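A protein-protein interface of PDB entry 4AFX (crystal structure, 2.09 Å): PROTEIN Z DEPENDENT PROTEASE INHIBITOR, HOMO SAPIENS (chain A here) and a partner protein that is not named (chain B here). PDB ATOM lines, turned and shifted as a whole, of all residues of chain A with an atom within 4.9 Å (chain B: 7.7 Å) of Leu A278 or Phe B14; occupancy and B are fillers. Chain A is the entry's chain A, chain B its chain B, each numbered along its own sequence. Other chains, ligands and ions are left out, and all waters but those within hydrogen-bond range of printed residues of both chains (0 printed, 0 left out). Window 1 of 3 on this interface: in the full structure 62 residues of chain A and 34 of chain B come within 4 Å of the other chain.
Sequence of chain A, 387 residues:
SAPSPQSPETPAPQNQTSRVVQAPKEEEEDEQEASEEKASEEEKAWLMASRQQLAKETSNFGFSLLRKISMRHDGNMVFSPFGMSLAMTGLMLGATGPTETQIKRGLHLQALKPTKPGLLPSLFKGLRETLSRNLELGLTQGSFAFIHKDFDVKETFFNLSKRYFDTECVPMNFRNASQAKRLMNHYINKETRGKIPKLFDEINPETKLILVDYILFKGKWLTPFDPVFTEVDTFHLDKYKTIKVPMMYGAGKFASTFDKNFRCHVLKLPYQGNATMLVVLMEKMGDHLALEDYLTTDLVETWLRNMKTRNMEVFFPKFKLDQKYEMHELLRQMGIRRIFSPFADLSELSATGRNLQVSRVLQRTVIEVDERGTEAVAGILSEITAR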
ATOM      1  N   MET A  77     -14.971  -6.420 -21.451  1.00  0.00           N
ATOM      2  CA  MET A  77     -14.222  -5.220 -21.104  1.00  0.00           C
ATOM      3  C   MET A  77     -15.049  -4.338 -20.197  1.00  0.00           C
ATOM      4  O   MET A  77     -16.274  -4.214 -20.391  1.00  0.00           O
ATOM      5  CB  MET A  77     -13.953  -4.401 -22.352  1.00  0.00           C
ATOM      6  CG  MET A  77     -12.869  -4.950 -23.279  1.00  0.00           C
ATOM      7  SD  MET A  77     -12.989  -4.052 -24.824  1.00  0.00           S
ATOM      8  CE  MET A  77     -11.326  -3.545 -24.976  1.00  0.00           C
ATOM      9  N   VAL A  78     -14.385  -3.702 -19.225  1.00  0.00           N
ATOM     10  CA  VAL A  78     -14.957  -2.624 -18.482  1.00  0.00           C
ATOM     11  C   VAL A  78     -13.886  -1.778 -17.828  1.00  0.00           C
ATOM     12  O   VAL A  78     -12.915  -2.305 -17.294  1.00  0.00           O
ATOM     13  CB  VAL A  78     -15.955  -3.106 -17.396  1.00  0.00           C
ATOM     14  CG1 VAL A  78     -15.292  -4.011 -16.350  1.00  0.00           C
ATOM     15  CG2 VAL A  78     -16.550  -1.948 -16.712  1.00  0.00           C
ATOM     16  N   VAL A 266     -30.225   1.023 -29.428  1.00  0.00           N
ATOM     17  CA  VAL A 266     -29.653   1.733 -28.282  1.00  0.00           C
ATOM     18  C   VAL A 266     -30.775   1.953 -27.272  1.00  0.00           C
ATOM     19  O   VAL A 266     -31.829   2.487 -27.621  1.00  0.00           O
ATOM     20  CB  VAL A 266     -29.073   3.088 -28.658  1.00  0.00           C
ATOM     21  CG1 VAL A 266     -28.369   3.699 -27.441  1.00  0.00           C
ATOM     22  CG2 VAL A 266     -28.127   2.965 -29.866  1.00  0.00           C
ATOM     23  N   LEU A 267     -30.541   1.546 -26.034  1.00  0.00           N
ATOM     24  CA  LEU A 267     -31.563   1.511 -25.016  1.00  0.00           C
ATOM     25  C   LEU A 267     -31.060   2.237 -23.761  1.00  0.00           C
ATOM     26  O   LEU A 267     -29.965   2.005 -23.340  1.00  0.00           O
ATOM     27  CB  LEU A 267     -31.877   0.042 -24.693  1.00  0.00           C
ATOM     28  CG  LEU A 267     -32.631  -0.186 -23.379  1.00  0.00           C
ATOM     29  CD1 LEU A 267     -34.042   0.357 -23.492  1.00  0.00           C
ATOM     30  CD2 LEU A 267     -32.624  -1.647 -22.924  1.00  0.00           C
ATOM     31  N   LYS A 268     -31.883   3.090 -23.158  1.00  0.00           N
ATOM     32  CA  LYS A 268     -31.561   3.709 -21.871  1.00  0.00           C
ATOM     33  C   LYS A 268     -32.166   2.892 -20.724  1.00  0.00           C
ATOM     34  O   LYS A 268     -33.341   2.528 -20.777  1.00  0.00           O
ATOM     35  CB  LYS A 268     -32.089   5.140 -21.806  1.00  0.00           C
ATOM     36  CG  LYS A 268     -31.320   6.137 -22.615  1.00  0.00           C
ATOM     37  CD  LYS A 268     -32.024   7.515 -22.682  1.00  0.00           C
ATOM     38  CE  LYS A 268     -31.867   8.353 -21.443  1.00  0.00           C
ATOM     39  NZ  LYS A 268     -32.416   9.733 -21.701  1.00  0.00           N
ATOM     40  N   THR A 276     -27.657   6.860 -15.670  1.00  0.00           N
ATOM     41  CA  THR A 276     -28.254   5.928 -16.605  1.00  0.00           C
ATOM     42  C   THR A 276     -27.180   5.052 -17.249  1.00  0.00           C
ATOM     43  O   THR A 276     -26.014   5.456 -17.399  1.00  0.00           O
ATOM     44  CB  THR A 276     -29.049   6.696 -17.700  1.00  0.00           C
ATOM     45  OG1 THR A 276     -29.762   5.779 -18.534  1.00  0.00           O
ATOM     46  CG2 THR A 276     -28.119   7.475 -18.566  1.00  0.00           C
ATOM     47  N   MET A 277     -27.588   3.835 -17.608  1.00  0.00           N
ATOM     48  CA  MET A 277     -26.790   2.945 -18.403  1.00  0.00           C
ATOM     49  C   MET A 277     -27.363   3.000 -19.826  1.00  0.00           C
ATOM     50  O   MET A 277     -28.561   2.873 -20.019  1.00  0.00           O
ATOM     51  CB  MET A 277     -26.888   1.516 -17.873  1.00  0.00           C
ATOM     52  CG  MET A 277     -26.117   0.519 -18.722  1.00  0.00           C
ATOM     53  SD  MET A 277     -26.133  -1.207 -18.187  1.00  0.00           S
ATOM     54  CE  MET A 277     -25.098  -1.134 -16.707  1.00  0.00           C
ATOM     55  N   LEU A 278     -26.489   3.172 -20.798  1.00  0.00           N
ATOM     56  CA  LEU A 278     -26.805   3.101 -22.198  1.00  0.00           C
ATOM     57  C   LEU A 278     -26.328   1.755 -22.618  1.00  0.00           C
ATOM     58  O   LEU A 278     -25.219   1.405 -22.299  1.00  0.00           O
ATOM     59  CB  LEU A 278     -25.984   4.098 -22.981  1.00  0.00           C
ATOM     60  CG  LEU A 278     -26.686   5.310 -23.523  1.00  0.00           C
ATOM     61  CD1 LEU A 278     -25.661   6.393 -23.863  1.00  0.00           C
ATOM     62  CD2 LEU A 278     -27.429   4.881 -24.717  1.00  0.00           C
ATOM     63  N   VAL A 279     -27.177   1.024 -23.325  1.00  0.00           N
ATOM     64  CA  VAL A 279     -26.855  -0.274 -23.867  1.00  0.00           C
ATOM     65  C   VAL A 279     -26.952  -0.165 -25.379  1.00  0.00           C
ATOM     66  O   VAL A 279     -27.940   0.343 -25.891  1.00  0.00           O
ATOM     67  CB  VAL A 279     -27.871  -1.308 -23.341  1.00  0.00           C
ATOM     68  CG1 VAL A 279     -27.624  -2.673 -23.972  1.00  0.00           C
ATOM     69  CG2 VAL A 279     -27.752  -1.371 -21.816  1.00  0.00           C
ATOM     70  N   VAL A 280     -25.905  -0.589 -26.078  1.00  0.00           N
ATOM     71  CA  VAL A 280     -25.870  -0.596 -27.534  1.00  0.00           C
ATOM     72  C   VAL A 280     -25.790  -2.049 -27.972  1.00  0.00           C
ATOM     73  O   VAL A 280     -24.849  -2.780 -27.583  1.00  0.00           O
ATOM     74  CB  VAL A 280     -24.652   0.185 -28.104  1.00  0.00           C
ATOM     75  CG1 VAL A 280     -24.633   0.100 -29.607  1.00  0.00           C
ATOM     76  CG2 VAL A 280     -24.678   1.644 -27.664  1.00  0.00           C
ATOM     77  N   VAL A 300     -23.064   9.386 -29.777  1.00  0.00           N
ATOM     78  CA  VAL A 300     -23.876   9.138 -28.602  1.00  0.00           C
ATOM     79  C   VAL A 300     -24.998  10.201 -28.515  1.00  0.00           C
ATOM     80  O   VAL A 300     -26.172   9.877 -28.301  1.00  0.00           O
ATOM     81  CB  VAL A 300     -22.997   9.120 -27.331  1.00  0.00           C
ATOM     82  CG1 VAL A 300     -23.831   9.168 -26.123  1.00  0.00           C
ATOM     83  CG2 VAL A 300     -22.126   7.854 -27.294  1.00  0.00           C
ATOM     84  N   LEU A 304     -29.154   9.949 -28.322  1.00  0.00           N
ATOM     85  CA  LEU A 304     -29.943  10.549 -27.221  1.00  0.00           C
ATOM     86  C   LEU A 304     -30.976  11.535 -27.762  1.00  0.00           C
ATOM     87  O   LEU A 304     -32.161  11.524 -27.354  1.00  0.00           O
ATOM     88  CB  LEU A 304     -29.021  11.226 -26.187  1.00  0.00           C
ATOM     89  CG  LEU A 304     -28.076  10.262 -25.471  1.00  0.00           C
ATOM     90  CD1 LEU A 304     -27.014  11.068 -24.678  1.00  0.00           C
ATOM     91  CD2 LEU A 304     -28.823   9.309 -24.580  1.00  0.00           C
ATOM     92  N   MET A 307     -33.995   9.439 -29.147  1.00  0.00           N
ATOM     93  CA  MET A 307     -34.704   8.496 -28.268  1.00  0.00           C
ATOM     94  C   MET A 307     -36.213   8.720 -28.304  1.00  0.00           C
ATOM     95  O   MET A 307     -36.671   9.861 -28.334  1.00  0.00           O
ATOM     96  CB  MET A 307     -34.267   8.694 -26.810  1.00  0.00           C
ATOM     97  CG  MET A 307     -32.904   8.217 -26.508  1.00  0.00           C
ATOM     98  SD  MET A 307     -32.787   6.447 -26.739  1.00  0.00           S
ATOM     99  CE  MET A 307     -31.038   6.275 -26.623  1.00  0.00           C
ATOM    100  N   PHE A 319     -25.005  -9.969 -15.245  1.00  0.00           N
ATOM    101  CA  PHE A 319     -23.591 -10.187 -15.492  1.00  0.00           C
ATOM    102  C   PHE A 319     -22.704  -9.645 -14.387  1.00  0.00           C
ATOM    103  O   PHE A 319     -23.118  -8.817 -13.613  1.00  0.00           O
ATOM    104  CB  PHE A 319     -23.154  -9.679 -16.877  1.00  0.00           C
ATOM    105  CG  PHE A 319     -23.261  -8.210 -17.087  1.00  0.00           C
ATOM    106  CD1 PHE A 319     -24.403  -7.652 -17.620  1.00  0.00           C
ATOM    107  CD2 PHE A 319     -22.166  -7.391 -16.853  1.00  0.00           C
ATOM    108  CE1 PHE A 319     -24.475  -6.301 -17.856  1.00  0.00           C
ATOM    109  CE2 PHE A 319     -22.237  -6.054 -17.079  1.00  0.00           C
ATOM    110  CZ  PHE A 319     -23.397  -5.502 -17.582  1.00  0.00           C
ATOM    111  N   LEU A 321     -18.455  -8.590 -14.151  1.00  0.00           N
ATOM    112  CA  LEU A 321     -17.155  -8.477 -14.803  1.00  0.00           C
ATOM    113  C   LEU A 321     -16.149  -8.076 -13.779  1.00  0.00           C
ATOM    114  O   LEU A 321     -16.491  -7.377 -12.798  1.00  0.00           O
ATOM    115  CB  LEU A 321     -17.157  -7.428 -15.902  1.00  0.00           C
ATOM    116  CG  LEU A 321     -18.197  -7.528 -17.025  1.00  0.00           C
ATOM    117  CD1 LEU A 321     -18.074  -6.342 -17.966  1.00  0.00           C
ATOM    118  CD2 LEU A 321     -18.072  -8.855 -17.775  1.00  0.00           C
ATOM    119  N   ILE A 367     -17.880  -4.912 -11.921  1.00  0.00           N
ATOM    120  CA  ILE A 367     -19.252  -4.454 -12.136  1.00  0.00           C
ATOM    121  C   ILE A 367     -20.166  -5.667 -11.981  1.00  0.00           C
ATOM    122  O   ILE A 367     -19.850  -6.765 -12.463  1.00  0.00           O
ATOM    123  CB  ILE A 367     -19.459  -3.743 -13.517  1.00  0.00           C
ATOM    124  CG1 ILE A 367     -20.899  -3.259 -13.662  1.00  0.00           C
ATOM    125  CG2 ILE A 367     -19.072  -4.657 -14.670  1.00  0.00           C
ATOM    126  CD1 ILE A 367     -21.136  -2.168 -14.734  1.00  0.00           C
ATOM    127  N   PHE B  12     -23.013  -6.813 -26.513  1.00  0.00           N
ATOM    128  CA  PHE B  12     -23.429  -5.452 -26.429  1.00  0.00           C
ATOM    129  C   PHE B  12     -22.379  -4.581 -25.775  1.00  0.00           C
ATOM    130  O   PHE B  12     -21.522  -5.067 -25.051  1.00  0.00           O
ATOM    131  CB  PHE B  12     -24.764  -5.382 -25.648  1.00  0.00           C
ATOM    132  CG  PHE B  12     -24.706  -5.918 -24.246  1.00  0.00           C
ATOM    133  CD1 PHE B  12     -24.950  -7.288 -23.976  1.00  0.00           C
ATOM    134  CD2 PHE B  12     -24.480  -5.054 -23.164  1.00  0.00           C
ATOM    135  CE1 PHE B  12     -24.895  -7.788 -22.682  1.00  0.00           C
ATOM    136  CE2 PHE B  12     -24.450  -5.566 -21.845  1.00  0.00           C
ATOM    137  CZ  PHE B  12     -24.655  -6.919 -21.614  1.00  0.00           C
ATOM    138  N   HIS B  13     -22.485  -3.282 -26.005  1.00  0.00           N
ATOM    139  CA  HIS B  13     -21.728  -2.289 -25.249  1.00  0.00           C
ATOM    140  C   HIS B  13     -22.586  -1.639 -24.192  1.00  0.00           C
ATOM    141  O   HIS B  13     -23.793  -1.673 -24.270  1.00  0.00           O
ATOM    142  CB  HIS B  13     -21.121  -1.268 -26.207  1.00  0.00           C
ATOM    143  CG  HIS B  13     -19.979  -1.813 -27.006  1.00  0.00           C
ATOM    144  ND1 HIS B  13     -20.158  -2.527 -28.172  1.00  0.00           N
ATOM    145  CD2 HIS B  13     -18.642  -1.750 -26.808  1.00  0.00           C
ATOM    146  CE1 HIS B  13     -18.984  -2.880 -28.653  1.00  0.00           C
ATOM    147  NE2 HIS B  13     -18.049  -2.402 -27.849  1.00  0.00           N
ATOM    148  N   PHE B  14     -21.960  -1.099 -23.151  1.00  0.00           N
ATOM    149  CA  PHE B  14     -22.697  -0.368 -22.157  1.00  0.00           C
ATOM    150  C   PHE B  14     -21.908   0.845 -21.691  1.00  0.00           C
ATOM    151  O   PHE B  14     -20.696   0.832 -21.712  1.00  0.00           O
ATOM    152  CB  PHE B  14     -23.103  -1.251 -20.978  1.00  0.00           C
ATOM    153  CG  PHE B  14     -21.952  -1.718 -20.152  1.00  0.00           C
ATOM    154  CD1 PHE B  14     -21.287  -2.896 -20.467  1.00  0.00           C
ATOM    155  CD2 PHE B  14     -21.514  -0.989 -19.067  1.00  0.00           C
ATOM    156  CE1 PHE B  14     -20.196  -3.338 -19.711  1.00  0.00           C
ATOM    157  CE2 PHE B  14     -20.429  -1.427 -18.294  1.00  0.00           C
ATOM    158  CZ  PHE B  14     -19.784  -2.611 -18.607  1.00  0.00           C
ATOM    159  N   MET B  15     -22.611   1.899 -21.309  1.00  0.00           N
ATOM    160  CA  MET B  15     -21.998   3.094 -20.729  1.00  0.00           C
ATOM    161  C   MET B  15     -22.852   3.503 -19.571  1.00  0.00           C
ATOM    162  O   MET B  15     -24.080   3.518 -19.729  1.00  0.00           O
ATOM    163  CB  MET B  15     -22.106   4.225 -21.708  1.00  0.00           C
ATOM    164  CG  MET B  15     -21.135   4.142 -22.798  1.00  0.00           C
ATOM    165  SD  MET B  15     -21.870   4.867 -24.249  1.00  0.00           S
ATOM    166  CE  MET B  15     -22.527   3.304 -24.853  1.00  0.00           C
ATOM    167  N   ILE B  16     -22.230   3.850 -18.440  1.00  0.00           N
ATOM    168  CA  ILE B  16     -22.931   4.402 -17.302  1.00  0.00           C
ATOM    169  C   ILE B  16     -22.511   5.871 -17.202  1.00  0.00           C
ATOM    170  O   ILE B  16     -21.296   6.170 -17.054  1.00  0.00           O
ATOM    171  CB  ILE B  16     -22.565   3.671 -16.008  1.00  0.00           C
ATOM    172  CG1 ILE B  16     -22.926   2.180 -16.135  1.00  0.00           C
ATOM    173  CG2 ILE B  16     -23.257   4.355 -14.786  1.00  0.00           C
ATOM    174  CD1 ILE B  16     -22.772   1.333 -14.847  1.00  0.00           C
ATOM    175  N   TYR B  17     -23.513   6.762 -17.322  1.00  0.00           N
ATOM    176  CA  TYR B  17     -23.357   8.210 -17.402  1.00  0.00           C
ATOM    177  C   TYR B  17     -24.041   8.883 -16.241  1.00  0.00           C
ATOM    178  O   TYR B  17     -25.134   8.489 -15.875  1.00  0.00           O
ATOM    179  CB  TYR B  17     -24.150   8.737 -18.600  1.00  0.00           C
ATOM    180  CG  TYR B  17     -23.418   8.722 -19.860  1.00  0.00           C
ATOM    181  CD1 TYR B  17     -22.492   9.708 -20.147  1.00  0.00           C
ATOM    182  CD2 TYR B  17     -23.633   7.702 -20.792  1.00  0.00           C
ATOM    183  CE1 TYR B  17     -21.776   9.701 -21.356  1.00  0.00           C
ATOM    184  CE2 TYR B  17     -22.916   7.671 -21.987  1.00  0.00           C
ATOM    185  CZ  TYR B  17     -21.993   8.676 -22.263  1.00  0.00           C
ATOM    186  OH  TYR B  17     -21.291   8.653 -23.444  1.00  0.00           O
ATOM    187  N   LEU B  24     -18.947  10.186 -18.028  1.00  0.00           N
ATOM    188  CA  LEU B  24     -18.980   8.766 -18.320  1.00  0.00           C
ATOM    189  C   LEU B  24     -18.217   8.045 -17.222  1.00  0.00           C
ATOM    190  O   LEU B  24     -16.985   8.136 -17.134  1.00  0.00           O
ATOM    191  CB  LEU B  24     -18.374   8.501 -19.711  1.00  0.00           C
ATOM    192  CG  LEU B  24     -18.421   7.076 -20.225  1.00  0.00           C
ATOM    193  CD1 LEU B  24     -19.825   6.509 -20.300  1.00  0.00           C
ATOM    194  CD2 LEU B  24     -17.730   7.002 -21.605  1.00  0.00           C
ATOM    195  N   PHE B  26     -18.470   4.613 -16.333  1.00  0.00           N
ATOM    196  CA  PHE B  26     -18.057   3.238 -16.650  1.00  0.00           C
ATOM    197  C   PHE B  26     -18.431   2.945 -18.102  1.00  0.00           C
ATOM    198  O   PHE B  26     -19.451   3.397 -18.588  1.00  0.00           O
ATOM    199  CB  PHE B  26     -18.752   2.216 -15.721  1.00  0.00           C
ATOM    200  CG  PHE B  26     -18.361   2.345 -14.284  1.00  0.00           C
ATOM    201  CD1 PHE B  26     -17.269   1.663 -13.790  1.00  0.00           C
ATOM    202  CD2 PHE B  26     -19.084   3.153 -13.422  1.00  0.00           C
ATOM    203  CE1 PHE B  26     -16.884   1.805 -12.456  1.00  0.00           C
ATOM    204  CE2 PHE B  26     -18.695   3.331 -12.100  1.00  0.00           C
ATOM    205  CZ  PHE B  26     -17.613   2.648 -11.608  1.00  0.00           C
ATOM    206  N   LEU B  27     -17.564   2.217 -18.786  1.00  0.00           N
ATOM    207  CA  LEU B  27     -17.694   1.926 -20.203  1.00  0.00           C
ATOM    208  C   LEU B  27     -17.225   0.501 -20.402  1.00  0.00           C
ATOM    209  O   LEU B  27     -16.194   0.122 -19.875  1.00  0.00           O
ATOM    210  CB  LEU B  27     -16.811   2.890 -20.987  1.00  0.00           C
ATOM    211  CG  LEU B  27     -16.722   2.693 -22.490  1.00  0.00           C
ATOM    212  CD1 LEU B  27     -18.071   2.972 -23.143  1.00  0.00           C
ATOM    213  CD2 LEU B  27     -15.629   3.602 -23.029  1.00  0.00           C
ATOM    214  N   GLY B  28     -17.997  -0.286 -21.147  1.00  0.00           N
ATOM    215  CA  GLY B  28     -17.599  -1.650 -21.419  1.00  0.00           C
ATOM    216  C   GLY B  28     -18.345  -2.349 -22.537  1.00  0.00           C
ATOM    217  O   GLY B  28     -19.132  -1.737 -23.290  1.00  0.00           O
ATOM    218  N   ARG B  29     -18.012  -3.630 -22.664  1.00  0.00           N
ATOM    219  CA  ARG B  29     -18.553  -4.535 -23.656  1.00  0.00           C
ATOM    220  C   ARG B  29     -18.716  -5.859 -22.962  1.00  0.00           C
ATOM    221  O   ARG B  29     -17.827  -6.279 -22.219  1.00  0.00           O
ATOM    222  CB  ARG B  29     -17.538  -4.736 -24.761  1.00  0.00           C
ATOM    223  CG  ARG B  29     -17.940  -5.716 -25.819  1.00  0.00           C
ATOM    224  CD  ARG B  29     -16.926  -5.693 -26.954  1.00  0.00           C
ATOM    225  NE  ARG B  29     -15.714  -6.451 -26.629  1.00  0.00           N
ATOM    226  CZ  ARG B  29     -14.575  -6.427 -27.333  1.00  0.00           C
ATOM    227  NH1 ARG B  29     -14.462  -5.680 -28.427  1.00  0.00           N
ATOM    228  NH2 ARG B  29     -13.535  -7.172 -26.944  1.00  0.00           N
ATOM    229  N   VAL B  30     -19.855  -6.503 -23.177  1.00  0.00           N
ATOM    230  CA  VAL B  30     -20.102  -7.868 -22.745  1.00  0.00           C
ATOM    231  C   VAL B  30     -20.275  -8.724 -24.028  1.00  0.00           C
ATOM    232  O   VAL B  30     -21.155  -8.465 -24.863  1.00  0.00           O
ATOM    233  CB  VAL B  30     -21.349  -7.937 -21.842  1.00  0.00           C
ATOM    234  CG1 VAL B  30     -21.689  -9.386 -21.464  1.00  0.00           C
ATOM    235  CG2 VAL B  30     -21.152  -7.023 -20.583  1.00  0.00           C
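O of Met A77 sits at hydrogen-bond distance from N of Arg B29, at 2.9 Å. O of Met B15 lies within hydrogen-bond range of N of Leu A278, at 2.7 Å. O of Val A280 is in hydrogen-bond range of N of His B13 (2.9 Å). N of Tyr B17 sits at hydrogen-bond distance from O of Thr A276.
N of Phe B14 sits at hydrogen-bond distance from O of Gly B28 (2.9 Å). N of Leu A321 lies within hydrogen-bond range of O of Ile A367 (2.9 Å). The backbone carbonyl oxygen of Phe B26 lies within hydrogen-bond range of the backbone NH of Ile B16 (2.8 Å). N of Val B30 sits at hydrogen-bond distance from O of Phe B12 (2.9 Å). N of Leu A267 is in hydrogen-bond range of O of Val A279, at 2.9 Å.
O of Leu B27 touches CA of Val A78, at 3.3 Å. Thr A276 touches Ile B16. Leu A278 touches Phe B14. O of His B13 touches CA of Val A279, at 3.4 Å. O of Val A280 touches CA of Phe B12 (3.2 Å). Val A280 touches Met B15. Val A300 touches Tyr B17 (CG1 to OH, 3.7 Å). Phe A319 touches Val B30. CD1 of Ile A367 touches CE2 of Phe B14 (3.7 Å). Ile A367 touches Ile B16.
Leu A278 touches four residues of chain B. Of chain A, only Val A78, Leu A278 and Ile A367 come within 4 Å of Phe B14. Printed residues of chain A within 4 Å of Gly B28: Met A77. Of the printed residues of chain A, His B13 touches Leu A278, Val A279 and Val A280. Printed residues of chain B within 4 Å of Val A279: His B13 (3.4 Å). Of the printed residues of chain A, Ile B16 touches Thr A276, Met A277 and Ile A367. Printed residues of chain A within 4 Å of Val B30: Phe A319. Leu A321 touches none of the printed residues of chain B. The nearest residue of chain B that does not touch Leu A278 is Ile B16 (4.9 Å). The nearest printed residue of chain A that does not touch Phe B14 is Leu A321 (4.1 Å). The nearest printed residue of chain A that does not touch Leu B27 is Met A77 (4.4 Å).
Hydrophobic or aromatic side chains of chain B within 4 Å of the printed part of chain A: Phe B12, Phe B14, Met B15, Ile B16, Tyr B17 and Val B30. Printed residues of chain A that touch a printed residue of chain B: Met A77, Val A78, Thr A276, Met A277, Leu A278, Val A279, Val A280, Val A300, Phe A319 and Ile A367. Along chain A the printed residues that touch a printed residue of chain B span positions 77 to 367. Among the printed residues, 22 pairs touch across the chains. Among the printed residues, no Asp or Glu carboxylate lies within 4 Å of a Lys or Arg side-chain nitrogen of the other chain.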
